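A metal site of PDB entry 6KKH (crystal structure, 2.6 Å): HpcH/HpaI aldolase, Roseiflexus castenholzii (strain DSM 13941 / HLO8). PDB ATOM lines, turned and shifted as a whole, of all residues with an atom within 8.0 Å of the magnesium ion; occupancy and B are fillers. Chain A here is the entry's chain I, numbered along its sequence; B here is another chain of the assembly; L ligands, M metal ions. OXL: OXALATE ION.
Merely in contact with the magnesium ion: Glu 59.
Four residues have an atom within 4 Å of the magnesium ion: Glu 59, Asp 60, Glu 156 and Asp 183.
The nearest printed residue that does not touch the magnesium ion is Lys 122 (4.4 Å).
The guanidinium group (NH2) of Arg 91 lies close to the backbone carbonyl oxygen (O) of Asp 60 (3.3 Å).
OE1 of Glu 156 lies within hydrogen-bond range of N of Lys 122 (3.3 Å).
The side-chain carboxylate (OE1) of Glu 59 lies within salt-bridge range of the guanidinium group (NH2) of Arg 91 (3.7 Å).
The side-chain amide oxygen (OD1) of Asn 57 is in hydrogen-bond range of the backbone NH (N) of Glu 59.
The backbone NH (N) of Leu 184 is in hydrogen-bond range of the backbone carbonyl oxygen (O) of Glu 156 (3.3 Å).
The side-chain amide nitrogen (ND2) of Asn 57 is in hydrogen-bond range of the backbone carbonyl oxygen (O) of Asp 60 (2.6 Å).
The magnesium ion is bound by OD2 of Asp 183 (2.1 Å), OE2 of Glu 156 (2.3 Å) and OD2 of Asp 60 (2.3 Å).
Slightly farther from the magnesium ion lies O4 of the ligand (2.8 Å).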
ATOM      1  N   ASN A  57     -12.432  -0.255  -6.721  1.00  0.00           N
ATOM      2  CA  ASN A  57     -11.087  -0.220  -6.115  1.00  0.00           C
ATOM      3  C   ASN A  57     -10.100  -0.955  -7.020  1.00  0.00           C
ATOM      4  O   ASN A  57     -10.359  -2.105  -7.319  1.00  0.00           O
ATOM      5  CB  ASN A  57     -11.092  -0.835  -4.725  1.00  0.00           C
ATOM      6  CG  ASN A  57      -9.774  -0.710  -3.993  1.00  0.00           C
ATOM      7  OD1 ASN A  57      -9.002   0.194  -4.262  1.00  0.00           O
ATOM      8  ND2 ASN A  57      -9.504  -1.608  -3.072  1.00  0.00           N
ATOM      9  N   GLU A  59      -6.420  -0.317  -6.290  1.00  0.00           N
ATOM     10  CA  GLU A  59      -5.077  -0.363  -5.635  1.00  0.00           C
ATOM     11  C   GLU A  59      -5.018  -1.279  -4.407  1.00  0.00           C
ATOM     12  O   GLU A  59      -4.816  -2.470  -4.611  1.00  0.00           O
ATOM     13  CB  GLU A  59      -4.278   0.953  -5.659  1.00  0.00           C
ATOM     14  CG  GLU A  59      -4.603   2.020  -4.606  1.00  0.00           C
ATOM     15  CD  GLU A  59      -3.610   2.134  -3.464  1.00  0.00           C
ATOM     16  OE1 GLU A  59      -4.055   2.228  -2.311  1.00  0.00           O
ATOM     17  OE2 GLU A  59      -2.405   2.189  -3.727  1.00  0.00           O
ATOM     18  N   ASP A  60      -5.105  -0.720  -3.199  1.00  0.00           N
ATOM     19  CA  ASP A  60      -4.934  -1.604  -2.025  1.00  0.00           C
ATOM     20  C   ASP A  60      -6.005  -2.699  -2.046  1.00  0.00           C
ATOM     21  O   ASP A  60      -7.088  -2.454  -2.618  1.00  0.00           O
ATOM     22  CB  ASP A  60      -4.811  -0.826  -0.708  1.00  0.00           C
ATOM     23  CG  ASP A  60      -3.395  -0.329  -0.446  1.00  0.00           C
ATOM     24  OD1 ASP A  60      -2.496  -0.718  -1.204  1.00  0.00           O
ATOM     25  OD2 ASP A  60      -3.212   0.446   0.511  1.00  0.00           O
ATOM     26  N   ALA A  61      -5.621  -3.878  -1.556  1.00  0.00           N
ATOM     27  CA  ALA A  61      -6.518  -5.049  -1.417  1.00  0.00           C
ATOM     28  C   ALA A  61      -6.663  -5.781  -2.741  1.00  0.00           C
ATOM     29  O   ALA A  61      -7.270  -6.845  -2.736  1.00  0.00           O
ATOM     30  CB  ALA A  61      -7.848  -4.597  -0.879  1.00  0.00           C
ATOM     31  N   ARG A  91     -11.065   4.218  -7.237  1.00  0.00           N
ATOM     32  CA  ARG A  91      -9.722   4.411  -6.699  1.00  0.00           C
ATOM     33  C   ARG A  91      -8.719   3.707  -7.625  1.00  0.00           C
ATOM     34  O   ARG A  91      -8.782   2.494  -7.808  1.00  0.00           O
ATOM     35  CB  ARG A  91      -9.614   3.899  -5.259  1.00  0.00           C
ATOM     36  CG  ARG A  91      -8.332   4.338  -4.549  1.00  0.00           C
ATOM     37  CD  ARG A  91      -8.255   3.921  -3.094  1.00  0.00           C
ATOM     38  NE  ARG A  91      -7.793   2.545  -2.909  1.00  0.00           N
ATOM     39  CZ  ARG A  91      -7.692   1.937  -1.732  1.00  0.00           C
ATOM     40  NH1 ARG A  91      -7.949   2.601  -0.613  1.00  0.00           N
ATOM     41  NH2 ARG A  91      -7.348   0.670  -1.662  1.00  0.00           N
ATOM     42  N   PRO A 121      -4.647   7.991  -4.497  1.00  0.00           N
ATOM     43  CA  PRO A 121      -4.036   7.542  -3.248  1.00  0.00           C
ATOM     44  C   PRO A 121      -2.589   8.003  -3.050  1.00  0.00           C
ATOM     45  O   PRO A 121      -1.893   8.295  -4.025  1.00  0.00           O
ATOM     46  CB  PRO A 121      -4.082   6.014  -3.377  1.00  0.00           C
ATOM     47  CG  PRO A 121      -3.760   5.798  -4.839  1.00  0.00           C
ATOM     48  CD  PRO A 121      -4.422   6.978  -5.537  1.00  0.00           C
ATOM     49  N   LYS A 122      -2.158   8.044  -1.791  1.00  0.00           N
ATOM     50  CA  LYS A 122      -0.787   8.403  -1.405  1.00  0.00           C
ATOM     51  C   LYS A 122      -0.403   9.760  -2.014  1.00  0.00           C
ATOM     52  O   LYS A 122       0.700   9.929  -2.525  1.00  0.00           O
ATOM     53  CB  LYS A 122       0.173   7.269  -1.809  1.00  0.00           C
ATOM     54  CG  LYS A 122       0.183   6.108  -0.831  1.00  0.00           C
ATOM     55  CD  LYS A 122       0.506   4.768  -1.445  1.00  0.00           C
ATOM     56  CE  LYS A 122       0.283   3.634  -0.469  1.00  0.00           C
ATOM     57  NZ  LYS A 122       0.674   2.322  -1.050  1.00  0.00           N
ATOM     58  N   LEU A 154      -6.714  11.157  -1.140  1.00  0.00           N
ATOM     59  CA  LEU A 154      -6.654  10.270   0.017  1.00  0.00           C
ATOM     60  C   LEU A 154      -5.478  10.693   0.901  1.00  0.00           C
ATOM     61  O   LEU A 154      -4.352  10.772   0.416  1.00  0.00           O
ATOM     62  CB  LEU A 154      -6.506   8.833  -0.486  1.00  0.00           C
ATOM     63  CG  LEU A 154      -6.723   7.720   0.540  1.00  0.00           C
ATOM     64  CD1 LEU A 154      -8.091   7.805   1.207  1.00  0.00           C
ATOM     65  CD2 LEU A 154      -6.537   6.355  -0.118  1.00  0.00           C
ATOM     66  N   LEU A 155      -5.748  10.967   2.177  1.00  0.00           N
ATOM     67  CA  LEU A 155      -4.715  11.319   3.167  1.00  0.00           C
ATOM     68  C   LEU A 155      -4.077  10.039   3.736  1.00  0.00           C
ATOM     69  O   LEU A 155      -4.586   9.480   4.704  1.00  0.00           O
ATOM     70  CB  LEU A 155      -5.361  12.137   4.294  1.00  0.00           C
ATOM     71  CG  LEU A 155      -6.072  13.418   3.865  1.00  0.00           C
ATOM     72  CD1 LEU A 155      -6.437  14.247   5.080  1.00  0.00           C
ATOM     73  CD2 LEU A 155      -5.205  14.237   2.909  1.00  0.00           C
ATOM     74  N   GLU A 156      -2.965   9.614   3.144  1.00  0.00           N
ATOM     75  CA  GLU A 156      -2.305   8.358   3.509  1.00  0.00           C
ATOM     76  C   GLU A 156      -0.878   8.601   4.027  1.00  0.00           C
ATOM     77  O   GLU A 156      -0.199   7.640   4.385  1.00  0.00           O
ATOM     78  CB  GLU A 156      -2.238   7.429   2.288  1.00  0.00           C
ATOM     79  CG  GLU A 156      -3.601   7.017   1.759  1.00  0.00           C
ATOM     80  CD  GLU A 156      -3.662   5.639   1.120  1.00  0.00           C
ATOM     81  OE1 GLU A 156      -3.111   5.469   0.014  1.00  0.00           O
ATOM     82  OE2 GLU A 156      -4.277   4.739   1.723  1.00  0.00           O
ATOM     83  N   GLY A 180      -7.153   7.931   5.167  1.00  0.00           N
ATOM     84  CA  GLY A 180      -6.745   6.529   5.056  1.00  0.00           C
ATOM     85  C   GLY A 180      -5.841   6.119   6.221  1.00  0.00           C
ATOM     86  O   GLY A 180      -4.633   6.306   6.131  1.00  0.00           O
ATOM     87  N   PRO A 181      -6.413   5.556   7.308  1.00  0.00           N
ATOM     88  CA  PRO A 181      -5.690   5.398   8.579  1.00  0.00           C
ATOM     89  C   PRO A 181      -4.586   4.335   8.572  1.00  0.00           C
ATOM     90  O   PRO A 181      -3.579   4.499   9.250  1.00  0.00           O
ATOM     91  CB  PRO A 181      -6.742   5.006   9.625  1.00  0.00           C
ATOM     92  CG  PRO A 181      -8.065   5.163   8.918  1.00  0.00           C
ATOM     93  CD  PRO A 181      -7.716   4.915   7.463  1.00  0.00           C
ATOM     94  N   ALA A 182      -4.786   3.241   7.843  1.00  0.00           N
ATOM     95  CA  ALA A 182      -3.801   2.169   7.820  1.00  0.00           C
ATOM     96  C   ALA A 182      -2.483   2.671   7.228  1.00  0.00           C
ATOM     97  O   ALA A 182      -1.407   2.288   7.678  1.00  0.00           O
ATOM     98  CB  ALA A 182      -4.334   0.994   7.049  1.00  0.00           C
ATOM     99  N   ASP A 183      -2.569   3.527   6.204  1.00  0.00           N
ATOM    100  CA  ASP A 183      -1.377   4.012   5.506  1.00  0.00           C
ATOM    101  C   ASP A 183      -0.814   5.213   6.253  1.00  0.00           C
ATOM    102  O   ASP A 183       0.402   5.394   6.303  1.00  0.00           O
ATOM    103  CB  ASP A 183      -1.681   4.393   4.047  1.00  0.00           C
ATOM    104  CG  ASP A 183      -1.243   3.354   3.022  1.00  0.00           C
ATOM    105  OD1 ASP A 183      -0.087   2.879   3.118  1.00  0.00           O
ATOM    106  OD2 ASP A 183      -2.069   3.033   2.138  1.00  0.00           O
ATOM    107  N   LEU A 184      -1.696   6.042   6.804  1.00  0.00           N
ATOM    108  CA  LEU A 184      -1.280   7.208   7.579  1.00  0.00           C
ATOM    109  C   LEU A 184      -0.512   6.753   8.830  1.00  0.00           C
ATOM    110  O   LEU A 184       0.428   7.410   9.252  1.00  0.00           O
ATOM    111  CB  LEU A 184      -2.501   8.038   7.969  1.00  0.00           C
ATOM    112  CG  LEU A 184      -2.199   9.380   8.639  1.00  0.00           C
ATOM    113  CD1 LEU A 184      -1.318  10.255   7.742  1.00  0.00           C
ATOM    114  CD2 LEU A 184      -3.472  10.123   8.993  1.00  0.00           C
ATOM    115  N   PRO A 245     -11.834   3.851   5.630  1.00  0.00           N
ATOM    116  CA  PRO A 245     -12.205   2.474   5.965  1.00  0.00           C
ATOM    117  C   PRO A 245     -12.247   2.186   7.476  1.00  0.00           C
ATOM    118  O   PRO A 245     -11.578   2.872   8.263  1.00  0.00           O
ATOM    119  CB  PRO A 245     -11.124   1.598   5.329  1.00  0.00           C
ATOM    120  CG  PRO A 245      -9.906   2.472   5.369  1.00  0.00           C
ATOM    121  CD  PRO A 245     -10.446   3.861   5.132  1.00  0.00           C
ATOM    122  N   TRP A 271     -16.498   5.188   4.574  1.00  0.00           N
ATOM    123  CA  TRP A 271     -16.333   4.087   3.621  1.00  0.00           C
ATOM    124  C   TRP A 271     -17.150   2.865   4.072  1.00  0.00           C
ATOM    125  O   TRP A 271     -17.518   2.749   5.252  1.00  0.00           O
ATOM    126  CB  TRP A 271     -14.860   3.705   3.470  1.00  0.00           C
ATOM    127  CG  TRP A 271     -14.022   4.714   2.741  1.00  0.00           C
ATOM    128  CD1 TRP A 271     -14.327   6.022   2.496  1.00  0.00           C
ATOM    129  CD2 TRP A 271     -12.724   4.492   2.170  1.00  0.00           C
ATOM    130  NE1 TRP A 271     -13.309   6.626   1.810  1.00  0.00           N
ATOM    131  CE2 TRP A 271     -12.316   5.704   1.587  1.00  0.00           C
ATOM    132  CE3 TRP A 271     -11.879   3.372   2.082  1.00  0.00           C
ATOM    133  CZ2 TRP A 271     -11.090   5.839   0.939  1.00  0.00           C
ATOM    134  CZ3 TRP A 271     -10.665   3.512   1.447  1.00  0.00           C
ATOM    135  CH2 TRP A 271     -10.278   4.725   0.876  1.00  0.00           C
ATOM    136  N   ASP B 317      -4.519  -5.415   3.990  1.00  0.00           N
ATOM    137  CA  ASP B 317      -4.120  -4.954   2.630  1.00  0.00           C
ATOM    138  C   ASP B 317      -2.644  -4.523   2.662  1.00  0.00           C
ATOM    139  O   ASP B 317      -1.938  -4.812   3.641  1.00  0.00           O
ATOM    140  CB  ASP B 317      -4.981  -3.792   2.146  1.00  0.00           C
ATOM    141  CG  ASP B 317      -5.031  -2.664   3.147  1.00  0.00           C
ATOM    142  OD1 ASP B 317      -4.544  -2.852   4.264  1.00  0.00           O
ATOM    143  OD2 ASP B 317      -5.557  -1.602   2.793  1.00  0.00           O
ATOM    144  N   ASP B 318      -2.210  -3.817   1.625  1.00  0.00           N
ATOM    145  CA  ASP B 318      -0.810  -3.346   1.536  1.00  0.00           C
ATOM    146  C   ASP B 318      -0.508  -2.413   2.713  1.00  0.00           C
ATOM    147  O   ASP B 318       0.576  -2.546   3.267  1.00  0.00           O
ATOM    148  CB  ASP B 318      -0.558  -2.626   0.218  1.00  0.00           C
ATOM    149  CG  ASP B 318      -1.120  -3.356  -0.976  1.00  0.00           C
ATOM    150  OD1 ASP B 318      -2.014  -4.179  -0.771  1.00  0.00           O
ATOM    151  OD2 ASP B 318      -0.670  -3.088  -2.082  1.00  0.00           O
ATOM    152  N   ALA B 319      -1.453  -1.558   3.101  1.00  0.00           N
ATOM    153  CA  ALA B 319      -1.212  -0.626   4.225  1.00  0.00           C
ATOM    154  C   ALA B 319      -0.905  -1.422   5.495  1.00  0.00           C
ATOM    155  O   ALA B 319       0.054  -1.081   6.172  1.00  0.00           O
ATOM    156  CB  ALA B 319      -2.425   0.233   4.403  1.00  0.00           C
ATOM    157  N   THR B 320      -1.661  -2.483   5.760  1.00  0.00           N
ATOM    158  CA  THR B 320      -1.374  -3.326   6.951  1.00  0.00           C
ATOM    159  C   THR B 320       0.005  -3.969   6.777  1.00  0.00           C
ATOM    160  O   THR B 320       0.685  -4.194   7.781  1.00  0.00           O
ATOM    161  CB  THR B 320      -2.535  -4.257   7.297  1.00  0.00           C
ATOM    162  OG1 THR B 320      -2.890  -4.892   6.070  1.00  0.00           O
ATOM    163  CG2 THR B 320      -3.728  -3.500   7.823  1.00  0.00           C
ATOM    164  N   LYS B 322       2.508  -2.613   5.342  1.00  0.00           N
ATOM    165  CA  LYS B 322       3.423  -1.510   5.684  1.00  0.00           C
ATOM    166  C   LYS B 322       3.437  -1.291   7.196  1.00  0.00           C
ATOM    167  O   LYS B 322       4.503  -1.204   7.796  1.00  0.00           O
ATOM    168  CB  LYS B 322       3.021  -0.233   4.936  1.00  0.00           C
ATOM    169  CG  LYS B 322       3.282  -0.254   3.434  1.00  0.00           C
ATOM    170  CD  LYS B 322       2.587   0.869   2.698  1.00  0.00           C
ATOM    171  CE  LYS B 322       2.792   0.801   1.192  1.00  0.00           C
ATOM    172  NZ  LYS B 322       2.059  -0.332   0.577  1.00  0.00           N
HETATM  173  C1  OXL L   1      -5.749   3.048   3.886  1.00  0.00           C
HETATM  174  C2  OXL L   1      -6.597   2.758   2.723  1.00  0.00           C
HETATM  175  O1  OXL L   1      -6.237   3.526   4.928  1.00  0.00           O
HETATM  176  O2  OXL L   1      -7.653   3.405   2.547  1.00  0.00           O
HETATM  177  O3  OXL L   1      -4.524   2.814   3.797  1.00  0.00           O
HETATM  178  O4  OXL L   1      -6.248   1.850   1.932  1.00  0.00           O
HETATM  179 MG    MG M   1      -3.760   2.687   0.914  1.00  0.00          MG
